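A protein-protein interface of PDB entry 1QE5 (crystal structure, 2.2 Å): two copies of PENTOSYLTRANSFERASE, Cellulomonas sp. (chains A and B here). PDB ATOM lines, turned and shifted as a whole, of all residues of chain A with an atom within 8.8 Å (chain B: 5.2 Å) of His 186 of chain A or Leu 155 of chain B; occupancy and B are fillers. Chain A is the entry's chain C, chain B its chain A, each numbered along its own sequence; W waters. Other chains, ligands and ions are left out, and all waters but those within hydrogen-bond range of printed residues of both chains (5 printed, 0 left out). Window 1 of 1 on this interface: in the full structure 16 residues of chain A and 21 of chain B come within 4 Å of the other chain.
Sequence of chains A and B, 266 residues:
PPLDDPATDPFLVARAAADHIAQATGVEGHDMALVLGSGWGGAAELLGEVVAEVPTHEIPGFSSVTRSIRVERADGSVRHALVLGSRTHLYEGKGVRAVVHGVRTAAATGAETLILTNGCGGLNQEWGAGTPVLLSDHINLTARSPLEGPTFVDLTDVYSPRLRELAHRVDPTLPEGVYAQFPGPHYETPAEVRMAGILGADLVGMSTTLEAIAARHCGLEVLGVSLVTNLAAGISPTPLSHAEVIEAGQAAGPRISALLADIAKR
The side-chain carboxylate (OD1) of Asp 137 of chain B sits close to the side-chain hydroxyl (OG1) of Thr 189 of chain A, 3.2 Å away. The side-chain carboxylate (OE2) of Glu 192 of chain A sits at hydrogen-bond distance from the backbone NH (N) of Asn 140 of chain B (2.8 Å). OD2 of Asp 137 of chain B lies within hydrogen-bond range of N of Ala 191 of chain A (3.0 Å). A ring nitrogen (ND1) of His 186 of chain A lies within hydrogen-bond range of the side-chain hydroxyl (OG) of Ser 145 of chain B (2.6 Å). The backbone carbonyl oxygen (O) of His 138 of chain B lies within hydrogen-bond range of the side-chain hydroxyl (OG1) of Thr 189 of chain A (2.9 Å).
No position is printed for both chains. Of the 23 pairs that touch across the chains among the printed residues, none has its exchanged pair printed and touching as well.
Of the 17 printed residues of chain A, 9 touch a printed residue of chain B. Hydrophobic or aromatic side chains of chain B that line the printed part of chain A: His 138, Leu 147, Leu 155, Val 158 and Ile 213. Among the printed residues, 23 pairs touch across the chains. Among the printed residues, no Asp or Glu carboxylate lies within 4 Å of a Lys or Arg side-chain nitrogen of the other chain.
Among the printed residues, pairs that only touch across the chains: Tyr 187 of chain A with Leu 155 of chain B, Gly 184 of chain A with Ser 145 of chain B, Tyr 187 of chain A with Val 153 of chain B, Pro 185 of chain A with Leu 147 of chain B, Pro 190 of chain A with Asp 137 of chain B, Pro 185 of chain A with Thr 151 of chain B, Pro 185 of chain A with Ser 145 of chain B, Ala 191 of chain A with His 138 of chain B, Ala 233 of chain A with Thr 156 of chain B, Pro 190 of chain A with Thr 156 of chain B, Pro 190 of chain A with Leu 155 of chain B, His 186 of chain A with Leu 155 of chain B, Thr 189 of chain A with Leu 155 of chain B, Glu 192 of chain A with His 138 of chain B, His 186 of chain A with Arg 144 of chain B, Thr 189 of chain A with Val 158 of chain B, His 186 of chain A with Leu 147 of chain B and His 186 of chain A with Ile 213 of chain B.
Of chain B, only Arg 144, Ser 145, Leu 147, Leu 155 and Ile 213 come within 4 Å of His 186 of chain A. No residue of chain A comes within 4 Å of Asp 154 of chain B. Of the printed residues of chain A, Ser 145 of chain B touches Gly 184, Pro 185 and His 186. Of the printed residues of chain B, Ala 191 of chain A touches Asp 137 and His 138. Of the printed residues of chain A, Asp 137 of chain B touches Thr 189 (3.0 Å), Pro 190 (3.5 Å) and Ala 191 (3.0 Å). Printed residues of chain A within 4 Å of Leu 147 of chain B: Pro 185 and His 186. Gly 205 of chain A touches none of the printed residues of chain B. The nearest residue of chain B that does not touch His 186 of chain A is Thr 151 of chain B (4.2 Å). The nearest printed residue of chain B that does not touch Pro 185 of chain A is Val 153 of chain B (5.3 Å).
The side-chain carboxylate of Glu 192 of chain A lies within hydrogen-bond range of the backbone NH of Thr 189 of chain A, at 2.8 Å. OD1 of Asp 154 of chain B lies within hydrogen-bond range of OG1 of Thr 156 of chain B, at 2.7 Å. N of Leu 147 of chain B sits close to OG of Ser 145 of chain B (3.2 Å). The side-chain hydroxyl of Thr 189 of chain A sits close to the backbone NH of Ala 191 of chain A, 3.4 Å away. ND2 of Asn 140 of chain B lies within hydrogen-bond range of O of Arg 144 of chain B (3.0 Å).
Water W5 lies within hydrogen-bond range of O of Leu 147 of chain B (2.6 Å) and O of Tyr 91 of chain A (3.1 Å). Water W4 lies within hydrogen-bond range of NE2 of His 186 of chain A (2.6 Å), ND2 of Asn 140 of chain B (2.7 Å) and OE2 of Glu 192 of chain A (3.1 Å). Water W2 lies within hydrogen-bond range of the backbone NH of Leu 155 of chain B (2.7 Å), the backbone carbonyl oxygen of Glu 188 of chain A (2.8 Å), the backbone NH of Thr 156 of chain B (3.2 Å) and the side-chain carboxylate of Asp 154 of chain B (3.3 Å). Water W1 lies within hydrogen-bond range of the backbone carbonyl oxygen (O) of Asn 140 of chain B (2.8 Å) and the side-chain carboxylate (OE2) of Glu 192 of chain A (2.8 Å). Water W3 bridges OE2 of Glu 192 of chain A and NE2 of His 138 of chain B.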
ATOM      1  N   TYR A  91      -3.178 -11.756   9.853  1.00  0.00           N
ATOM      2  CA  TYR A  91      -3.989 -12.268  10.958  1.00  0.00           C
ATOM      3  C   TYR A  91      -3.219 -12.936  12.064  1.00  0.00           C
ATOM      4  O   TYR A  91      -3.811 -13.522  12.985  1.00  0.00           O
ATOM      5  CB  TYR A  91      -5.062 -13.217  10.445  1.00  0.00           C
ATOM      6  CG  TYR A  91      -4.547 -14.497   9.828  1.00  0.00           C
ATOM      7  CD1 TYR A  91      -3.784 -15.392  10.578  1.00  0.00           C
ATOM      8  CD2 TYR A  91      -4.856 -14.826   8.493  1.00  0.00           C
ATOM      9  CE1 TYR A  91      -3.326 -16.582  10.031  1.00  0.00           C
ATOM     10  CE2 TYR A  91      -4.406 -16.010   7.928  1.00  0.00           C
ATOM     11  CZ  TYR A  91      -3.629 -16.885   8.708  1.00  0.00           C
ATOM     12  OH  TYR A  91      -3.078 -18.018   8.128  1.00  0.00           O
ATOM     13  N   PHE A 182      -8.894  -9.835   2.174  1.00  0.00           N
ATOM     14  CA  PHE A 182      -9.676  -9.644   3.397  1.00  0.00           C
ATOM     15  C   PHE A 182      -8.714  -9.898   4.529  1.00  0.00           C
ATOM     16  O   PHE A 182      -7.757 -10.641   4.387  1.00  0.00           O
ATOM     17  CB  PHE A 182     -10.812 -10.671   3.508  1.00  0.00           C
ATOM     18  CG  PHE A 182     -12.036 -10.304   2.701  1.00  0.00           C
ATOM     19  CD1 PHE A 182     -12.152 -10.669   1.364  1.00  0.00           C
ATOM     20  CD2 PHE A 182     -13.077  -9.549   3.280  1.00  0.00           C
ATOM     21  CE1 PHE A 182     -13.270 -10.293   0.608  1.00  0.00           C
ATOM     22  CE2 PHE A 182     -14.212  -9.173   2.525  1.00  0.00           C
ATOM     23  CZ  PHE A 182     -14.300  -9.545   1.197  1.00  0.00           C
ATOM     24  N   PRO A 183      -8.885  -9.210   5.639  1.00  0.00           N
ATOM     25  CA  PRO A 183      -7.928  -9.520   6.693  1.00  0.00           C
ATOM     26  C   PRO A 183      -7.864 -10.941   7.195  1.00  0.00           C
ATOM     27  O   PRO A 183      -6.767 -11.442   7.535  1.00  0.00           O
ATOM     28  CB  PRO A 183      -8.269  -8.495   7.790  1.00  0.00           C
ATOM     29  CG  PRO A 183      -9.596  -8.036   7.449  1.00  0.00           C
ATOM     30  CD  PRO A 183      -9.681  -8.031   5.984  1.00  0.00           C
ATOM     31  N   GLY A 184      -9.003 -11.631   7.214  1.00  0.00           N
ATOM     32  CA  GLY A 184      -9.034 -12.985   7.738  1.00  0.00           C
ATOM     33  C   GLY A 184      -8.833 -13.007   9.248  1.00  0.00           C
ATOM     34  O   GLY A 184      -8.766 -11.945   9.875  1.00  0.00           O
ATOM     35  N   PRO A 185      -8.649 -14.198   9.872  1.00  0.00           N
ATOM     36  CA  PRO A 185      -8.590 -15.572   9.338  1.00  0.00           C
ATOM     37  C   PRO A 185      -9.932 -16.275   9.012  1.00  0.00           C
ATOM     38  O   PRO A 185      -9.974 -17.285   8.264  1.00  0.00           O
ATOM     39  CB  PRO A 185      -7.802 -16.296  10.429  1.00  0.00           C
ATOM     40  CG  PRO A 185      -8.378 -15.652  11.713  1.00  0.00           C
ATOM     41  CD  PRO A 185      -8.321 -14.169  11.318  1.00  0.00           C
ATOM     42  N   HIS A 186     -11.038 -15.764   9.582  1.00  0.00           N
ATOM     43  CA  HIS A 186     -12.342 -16.353   9.322  1.00  0.00           C
ATOM     44  C   HIS A 186     -12.619 -16.115   7.830  1.00  0.00           C
ATOM     45  O   HIS A 186     -12.032 -15.216   7.231  1.00  0.00           O
ATOM     46  CB  HIS A 186     -13.403 -15.654  10.212  1.00  0.00           C
ATOM     47  CG  HIS A 186     -13.576 -14.189   9.919  1.00  0.00           C
ATOM     48  ND1 HIS A 186     -12.898 -13.197  10.602  1.00  0.00           N
ATOM     49  CD2 HIS A 186     -14.308 -13.557   8.978  1.00  0.00           C
ATOM     50  CE1 HIS A 186     -13.209 -12.014  10.089  1.00  0.00           C
ATOM     51  NE2 HIS A 186     -14.064 -12.203   9.105  1.00  0.00           N
ATOM     52  N   TYR A 187     -13.487 -16.929   7.228  1.00  0.00           N
ATOM     53  CA  TYR A 187     -13.852 -16.814   5.831  1.00  0.00           C
ATOM     54  C   TYR A 187     -15.018 -15.869   5.650  1.00  0.00           C
ATOM     55  O   TYR A 187     -15.640 -15.448   6.613  1.00  0.00           O
ATOM     56  CB  TYR A 187     -14.215 -18.165   5.257  1.00  0.00           C
ATOM     57  CG  TYR A 187     -13.009 -19.048   5.100  1.00  0.00           C
ATOM     58  CD1 TYR A 187     -12.142 -18.858   4.018  1.00  0.00           C
ATOM     59  CD2 TYR A 187     -12.689 -20.031   6.047  1.00  0.00           C
ATOM     60  CE1 TYR A 187     -10.983 -19.606   3.858  1.00  0.00           C
ATOM     61  CE2 TYR A 187     -11.516 -20.804   5.899  1.00  0.00           C
ATOM     62  CZ  TYR A 187     -10.674 -20.574   4.792  1.00  0.00           C
ATOM     63  OH  TYR A 187      -9.527 -21.314   4.598  1.00  0.00           O
ATOM     64  N   GLU A 188     -15.314 -15.543   4.410  1.00  0.00           N
ATOM     65  CA  GLU A 188     -16.385 -14.641   4.094  1.00  0.00           C
ATOM     66  C   GLU A 188     -17.780 -15.284   4.123  1.00  0.00           C
ATOM     67  O   GLU A 188     -17.954 -16.436   3.744  1.00  0.00           O
ATOM     68  CB  GLU A 188     -16.138 -14.015   2.712  1.00  0.00           C
ATOM     69  CG  GLU A 188     -14.898 -13.101   2.656  1.00  0.00           C
ATOM     70  CD  GLU A 188     -13.579 -13.871   2.934  1.00  0.00           C
ATOM     71  OE1 GLU A 188     -13.396 -14.961   2.372  1.00  0.00           O
ATOM     72  OE2 GLU A 188     -12.722 -13.391   3.727  1.00  0.00           O
ATOM     73  N   THR A 189     -18.785 -14.510   4.551  1.00  0.00           N
ATOM     74  CA  THR A 189     -20.149 -15.002   4.572  1.00  0.00           C
ATOM     75  C   THR A 189     -20.663 -14.844   3.148  1.00  0.00           C
ATOM     76  O   THR A 189     -20.072 -14.100   2.355  1.00  0.00           O
ATOM     77  CB  THR A 189     -21.112 -14.105   5.452  1.00  0.00           C
ATOM     78  OG1 THR A 189     -21.145 -12.765   4.918  1.00  0.00           O
ATOM     79  CG2 THR A 189     -20.695 -14.077   6.863  1.00  0.00           C
ATOM     80  N   PRO A 190     -21.719 -15.598   2.778  1.00  0.00           N
ATOM     81  CA  PRO A 190     -22.242 -15.421   1.426  1.00  0.00           C
ATOM     82  C   PRO A 190     -22.499 -13.892   1.085  1.00  0.00           C
ATOM     83  O   PRO A 190     -22.260 -13.438  -0.067  1.00  0.00           O
ATOM     84  CB  PRO A 190     -23.531 -16.259   1.460  1.00  0.00           C
ATOM     85  CG  PRO A 190     -23.077 -17.453   2.364  1.00  0.00           C
ATOM     86  CD  PRO A 190     -22.408 -16.705   3.500  1.00  0.00           C
ATOM     87  N   ALA A 191     -22.973 -13.094   2.064  1.00  0.00           N
ATOM     88  CA  ALA A 191     -23.208 -11.668   1.785  1.00  0.00           C
ATOM     89  C   ALA A 191     -21.871 -10.958   1.542  1.00  0.00           C
ATOM     90  O   ALA A 191     -21.807 -10.031   0.752  1.00  0.00           O
ATOM     91  CB  ALA A 191     -23.968 -10.968   2.926  1.00  0.00           C
ATOM     92  N   GLU A 192     -20.823 -11.352   2.241  1.00  0.00           N
ATOM     93  CA  GLU A 192     -19.508 -10.693   2.000  1.00  0.00           C
ATOM     94  C   GLU A 192     -18.905 -11.082   0.606  1.00  0.00           C
ATOM     95  O   GLU A 192     -18.251 -10.283  -0.070  1.00  0.00           O
ATOM     96  CB  GLU A 192     -18.566 -11.029   3.145  1.00  0.00           C
ATOM     97  CG  GLU A 192     -18.937 -10.281   4.410  1.00  0.00           C
ATOM     98  CD  GLU A 192     -18.298 -10.848   5.613  1.00  0.00           C
ATOM     99  OE1 GLU A 192     -17.974 -12.052   5.572  1.00  0.00           O
ATOM    100  OE2 GLU A 192     -18.132 -10.105   6.596  1.00  0.00           O
ATOM    101  N   VAL A 193     -19.213 -12.288   0.181  1.00  0.00           N
ATOM    102  CA  VAL A 193     -18.791 -12.789  -1.102  1.00  0.00           C
ATOM    103  C   VAL A 193     -19.544 -12.078  -2.200  1.00  0.00           C
ATOM    104  O   VAL A 193     -18.943 -11.781  -3.239  1.00  0.00           O
ATOM    105  CB  VAL A 193     -18.953 -14.300  -1.131  1.00  0.00           C
ATOM    106  CG1 VAL A 193     -18.855 -14.850  -2.547  1.00  0.00           C
ATOM    107  CG2 VAL A 193     -17.856 -14.881  -0.276  1.00  0.00           C
ATOM    108  N   GLY A 205      -9.188 -13.911  -0.754  1.00  0.00           N
ATOM    109  CA  GLY A 205      -8.273 -14.649   0.053  1.00  0.00           C
ATOM    110  C   GLY A 205      -7.694 -13.705   1.077  1.00  0.00           C
ATOM    111  O   GLY A 205      -8.163 -12.569   1.253  1.00  0.00           O
ATOM    112  N   MET A 206      -6.617 -14.138   1.704  1.00  0.00           N
ATOM    113  CA  MET A 206      -6.026 -13.399   2.800  1.00  0.00           C
ATOM    114  C   MET A 206      -4.601 -12.973   2.758  1.00  0.00           C
ATOM    115  O   MET A 206      -3.941 -12.846   3.842  1.00  0.00           O
ATOM    116  CB  MET A 206      -6.211 -14.268   4.050  1.00  0.00           C
ATOM    117  CG  MET A 206      -7.676 -14.745   4.215  1.00  0.00           C
ATOM    118  SD  MET A 206      -7.876 -15.998   5.515  1.00  0.00           S
ATOM    119  CE  MET A 206      -9.662 -16.228   5.269  1.00  0.00           C
ATOM    120  N   ALA A 233     -18.131 -19.009  -0.433  1.00  0.00           N
ATOM    121  CA  ALA A 233     -19.502 -19.215   0.143  1.00  0.00           C
ATOM    122  C   ALA A 233     -20.647 -18.647  -0.724  1.00  0.00           C
ATOM    123  O   ALA A 233     -20.570 -17.509  -1.239  1.00  0.00           O
ATOM    124  CB  ALA A 233     -19.570 -18.627   1.545  1.00  0.00           C
ATOM    125  N   GLY A 234     -21.651 -19.506  -0.941  1.00  0.00           N
ATOM    126  CA  GLY A 234     -22.831 -19.180  -1.726  1.00  0.00           C
ATOM    127  C   GLY A 234     -22.673 -19.183  -3.227  1.00  0.00           C
ATOM    128  O   GLY A 234     -23.632 -18.942  -3.948  1.00  0.00           O
ATOM    129  N   ASP B 137     -27.939 -12.710   7.500  1.00  0.00           N
ATOM    130  CA  ASP B 137     -26.485 -12.763   7.199  1.00  0.00           C
ATOM    131  C   ASP B 137     -25.961 -11.379   7.600  1.00  0.00           C
ATOM    132  O   ASP B 137     -26.758 -10.458   7.954  1.00  0.00           O
ATOM    133  CB  ASP B 137     -26.255 -12.958   5.656  1.00  0.00           C
ATOM    134  CG  ASP B 137     -24.892 -13.659   5.295  1.00  0.00           C
ATOM    135  OD1 ASP B 137     -23.974 -13.692   6.127  1.00  0.00           O
ATOM    136  OD2 ASP B 137     -24.756 -14.169   4.165  1.00  0.00           O
ATOM    137  N   HIS B 138     -24.635 -11.222   7.545  1.00  0.00           N
ATOM    138  CA  HIS B 138     -24.013  -9.926   7.839  1.00  0.00           C
ATOM    139  C   HIS B 138     -22.840  -9.628   6.918  1.00  0.00           C
ATOM    140  O   HIS B 138     -22.411 -10.471   6.117  1.00  0.00           O
ATOM    141  CB  HIS B 138     -23.556  -9.855   9.285  1.00  0.00           C
ATOM    142  CG  HIS B 138     -22.435 -10.776   9.628  1.00  0.00           C
ATOM    143  ND1 HIS B 138     -22.474 -11.597  10.736  1.00  0.00           N
ATOM    144  CD2 HIS B 138     -21.204 -10.944   9.064  1.00  0.00           C
ATOM    145  CE1 HIS B 138     -21.320 -12.237  10.841  1.00  0.00           C
ATOM    146  NE2 HIS B 138     -20.528 -11.859   9.843  1.00  0.00           N
ATOM    147  N   ASN B 140     -19.184  -7.685   7.613  1.00  0.00           N
ATOM    148  CA  ASN B 140     -18.328  -7.068   8.628  1.00  0.00           C
ATOM    149  C   ASN B 140     -17.466  -6.037   7.953  1.00  0.00           C
ATOM    150  O   ASN B 140     -16.650  -6.393   7.067  1.00  0.00           O
ATOM    151  CB  ASN B 140     -17.487  -8.163   9.266  1.00  0.00           C
ATOM    152  CG  ASN B 140     -16.413  -7.635  10.172  1.00  0.00           C
ATOM    153  OD1 ASN B 140     -16.327  -6.464  10.495  1.00  0.00           O
ATOM    154  ND2 ASN B 140     -15.587  -8.527  10.602  1.00  0.00           N
ATOM    155  N   ARG B 144     -11.736  -6.087  11.117  1.00  0.00           N
ATOM    156  CA  ARG B 144     -11.172  -6.782  12.271  1.00  0.00           C
ATOM    157  C   ARG B 144     -11.786  -8.162  12.315  1.00  0.00           C
ATOM    158  O   ARG B 144     -12.735  -8.453  11.601  1.00  0.00           O
ATOM    159  CB  ARG B 144     -11.441  -6.036  13.588  1.00  0.00           C
ATOM    160  CG  ARG B 144     -11.175  -4.523  13.571  1.00  0.00           C
ATOM    161  CD  ARG B 144      -9.730  -4.150  13.530  1.00  0.00           C
ATOM    162  NE  ARG B 144      -9.044  -4.733  14.673  1.00  0.00           N
ATOM    163  CZ  ARG B 144      -9.083  -4.237  15.918  1.00  0.00           C
ATOM    164  NH1 ARG B 144      -9.778  -3.115  16.190  1.00  0.00           N
ATOM    165  NH2 ARG B 144      -8.452  -4.880  16.902  1.00  0.00           N
ATOM    166  N   SER B 145     -11.187  -9.034  13.126  1.00  0.00           N
ATOM    167  CA  SER B 145     -11.634 -10.386  13.296  1.00  0.00           C
ATOM    168  C   SER B 145     -11.392 -10.734  14.727  1.00  0.00           C
ATOM    169  O   SER B 145     -10.500 -10.210  15.347  1.00  0.00           O
ATOM    170  CB  SER B 145     -10.820 -11.339  12.446  1.00  0.00           C
ATOM    171  OG  SER B 145     -11.269 -12.684  12.601  1.00  0.00           O
ATOM    172  N   PRO B 146     -12.278 -11.529  15.313  1.00  0.00           N
ATOM    173  CA  PRO B 146     -12.054 -11.916  16.707  1.00  0.00           C
ATOM    174  C   PRO B 146     -11.148 -13.145  16.754  1.00  0.00           C
ATOM    175  O   PRO B 146     -10.715 -13.554  17.807  1.00  0.00           O
ATOM    176  CB  PRO B 146     -13.473 -12.208  17.195  1.00  0.00           C
ATOM    177  CG  PRO B 146     -14.093 -12.914  15.950  1.00  0.00           C
ATOM    178  CD  PRO B 146     -13.617 -11.945  14.835  1.00  0.00           C
ATOM    179  N   LEU B 147     -10.903 -13.770  15.616  1.00  0.00           N
ATOM    180  CA  LEU B 147     -10.072 -14.969  15.590  1.00  0.00           C
ATOM    181  C   LEU B 147      -8.618 -14.597  15.482  1.00  0.00           C
ATOM    182  O   LEU B 147      -8.256 -13.651  14.776  1.00  0.00           O
ATOM    183  CB  LEU B 147     -10.457 -15.895  14.460  1.00  0.00           C
ATOM    184  CG  LEU B 147     -11.911 -16.296  14.606  1.00  0.00           C
ATOM    185  CD1 LEU B 147     -12.216 -17.334  13.552  1.00  0.00           C
ATOM    186  CD2 LEU B 147     -12.194 -16.842  16.019  1.00  0.00           C
ATOM    187  N   THR B 151      -7.479 -19.995  12.021  1.00  0.00           N
ATOM    188  CA  THR B 151      -8.687 -20.489  12.564  1.00  0.00           C
ATOM    189  C   THR B 151      -9.567 -20.561  11.356  1.00  0.00           C
ATOM    190  O   THR B 151     -10.157 -19.593  10.923  1.00  0.00           O
ATOM    191  CB  THR B 151      -9.153 -19.520  13.660  1.00  0.00           C
ATOM    192  OG1 THR B 151      -8.041 -19.200  14.529  1.00  0.00           O
ATOM    193  CG2 THR B 151     -10.231 -20.153  14.502  1.00  0.00           C
ATOM    194  N   VAL B 153     -12.643 -21.393  10.202  1.00  0.00           N
ATOM    195  CA  VAL B 153     -14.097 -21.483  10.465  1.00  0.00           C
ATOM    196  C   VAL B 153     -14.984 -21.029   9.289  1.00  0.00           C
ATOM    197  O   VAL B 153     -14.792 -19.939   8.685  1.00  0.00           O
ATOM    198  CB  VAL B 153     -14.507 -20.625  11.714  1.00  0.00           C
ATOM    199  CG1 VAL B 153     -13.429 -19.649  12.065  1.00  0.00           C
ATOM    200  CG2 VAL B 153     -15.762 -19.811  11.432  1.00  0.00           C
ATOM    201  N   ASP B 154     -15.987 -21.868   9.021  1.00  0.00           N
ATOM    202  CA  ASP B 154     -16.951 -21.664   7.944  1.00  0.00           C
ATOM    203  C   ASP B 154     -18.093 -20.719   8.420  1.00  0.00           C
ATOM    204  O   ASP B 154     -18.681 -20.944   9.464  1.00  0.00           O
ATOM    205  CB  ASP B 154     -17.527 -23.028   7.583  1.00  0.00           C
ATOM    206  CG  ASP B 154     -18.650 -22.931   6.591  1.00  0.00           C
ATOM    207  OD1 ASP B 154     -18.655 -21.943   5.826  1.00  0.00           O
ATOM    208  OD2 ASP B 154     -19.525 -23.820   6.563  1.00  0.00           O
ATOM    209  N   LEU B 155     -18.357 -19.640   7.685  1.00  0.00           N
ATOM    210  CA  LEU B 155     -19.426 -18.707   8.052  1.00  0.00           C
ATOM    211  C   LEU B 155     -20.573 -18.775   7.007  1.00  0.00           C
ATOM    212  O   LEU B 155     -21.343 -17.842   6.815  1.00  0.00           O
ATOM    213  CB  LEU B 155     -18.907 -17.267   8.128  1.00  0.00           C
ATOM    214  CG  LEU B 155     -17.736 -17.055   9.069  1.00  0.00           C
ATOM    215  CD1 LEU B 155     -17.404 -15.562   9.150  1.00  0.00           C
ATOM    216  CD2 LEU B 155     -18.063 -17.620  10.434  1.00  0.00           C
ATOM    217  N   THR B 156     -20.711 -19.910   6.343  1.00  0.00           N
ATOM    218  CA  THR B 156     -21.752 -20.045   5.336  1.00  0.00           C
ATOM    219  C   THR B 156     -23.169 -19.926   5.873  1.00  0.00           C
ATOM    220  O   THR B 156     -24.093 -19.638   5.105  1.00  0.00           O
ATOM    221  CB  THR B 156     -21.606 -21.341   4.605  1.00  0.00           C
ATOM    222  OG1 THR B 156     -20.371 -21.293   3.886  1.00  0.00           O
ATOM    223  CG2 THR B 156     -22.755 -21.539   3.649  1.00  0.00           C
ATOM    224  N   ASP B 157     -23.349 -20.175   7.174  1.00  0.00           N
ATOM    225  CA  ASP B 157     -24.668 -20.018   7.782  1.00  0.00           C
ATOM    226  C   ASP B 157     -24.512 -19.575   9.211  1.00  0.00           C
ATOM    227  O   ASP B 157     -24.798 -20.304  10.170  1.00  0.00           O
ATOM    228  CB  ASP B 157     -25.513 -21.298   7.665  1.00  0.00           C
ATOM    229  CG  ASP B 157     -26.732 -21.099   6.715  1.00  0.00           C
ATOM    230  OD1 ASP B 157     -27.497 -20.111   6.934  1.00  0.00           O
ATOM    231  OD2 ASP B 157     -26.921 -21.909   5.763  1.00  0.00           O
ATOM    232  N   VAL B 158     -24.024 -18.356   9.332  1.00  0.00           N
ATOM    233  CA  VAL B 158     -23.794 -17.793  10.631  1.00  0.00           C
ATOM    234  C   VAL B 158     -25.087 -17.742  11.456  1.00  0.00           C
ATOM    235  O   VAL B 158     -25.085 -18.108  12.638  1.00  0.00           O
ATOM    236  CB  VAL B 158     -23.243 -16.387  10.519  1.00  0.00           C
ATOM    237  CG1 VAL B 158     -23.135 -15.743  11.938  1.00  0.00           C
ATOM    238  CG2 VAL B 158     -21.889 -16.419   9.759  1.00  0.00           C
ATOM    239  N   ILE B 213     -19.173 -14.215  14.960  1.00  0.00           N
ATOM    240  CA  ILE B 213     -18.043 -14.990  14.420  1.00  0.00           C
ATOM    241  C   ILE B 213     -17.440 -15.723  15.589  1.00  0.00           C
ATOM    242  O   ILE B 213     -17.274 -16.919  15.553  1.00  0.00           O
ATOM    243  CB  ILE B 213     -16.990 -14.055  13.719  1.00  0.00           C
ATOM    244  CG1 ILE B 213     -17.631 -13.408  12.482  1.00  0.00           C
ATOM    245  CG2 ILE B 213     -15.775 -14.889  13.249  1.00  0.00           C
ATOM    246  CD1 ILE B 213     -16.899 -12.209  11.996  1.00  0.00           C
ATOM    247  N   ARG B 216     -19.808 -18.746  16.483  1.00  0.00           N
ATOM    248  CA  ARG B 216     -19.774 -19.876  15.579  1.00  0.00           C
ATOM    249  C   ARG B 216     -18.425 -20.619  15.721  1.00  0.00           C
ATOM    250  O   ARG B 216     -18.332 -21.823  15.570  1.00  0.00           O
ATOM    251  CB  ARG B 216     -19.926 -19.374  14.167  1.00  0.00           C
ATOM    252  CG  ARG B 216     -21.216 -18.674  13.882  1.00  0.00           C
ATOM    253  CD  ARG B 216     -22.088 -19.643  13.104  1.00  0.00           C
ATOM    254  NE  ARG B 216     -22.331 -20.733  13.978  1.00  0.00           N
ATOM    255  CZ  ARG B 216     -22.415 -22.013  13.662  1.00  0.00           C
ATOM    256  NH1 ARG B 216     -22.285 -22.444  12.413  1.00  0.00           N
ATOM    257  NH2 ARG B 216     -22.640 -22.855  14.666  1.00  0.00           N
HETATM  258  O   HOH W   1     -16.066  -8.566   5.395  1.00  0.00           O
HETATM  259  O   HOH W   2     -17.919 -18.777   5.199  1.00  0.00           O
HETATM  260  O   HOH W   3     -17.918 -12.137   8.529  1.00  0.00           O
HETATM  261  O   HOH W   4     -16.100 -10.567   8.886  1.00  0.00           O
HETATM  262  O   HOH W   5      -6.432 -12.133  13.735  1.00  0.00           O
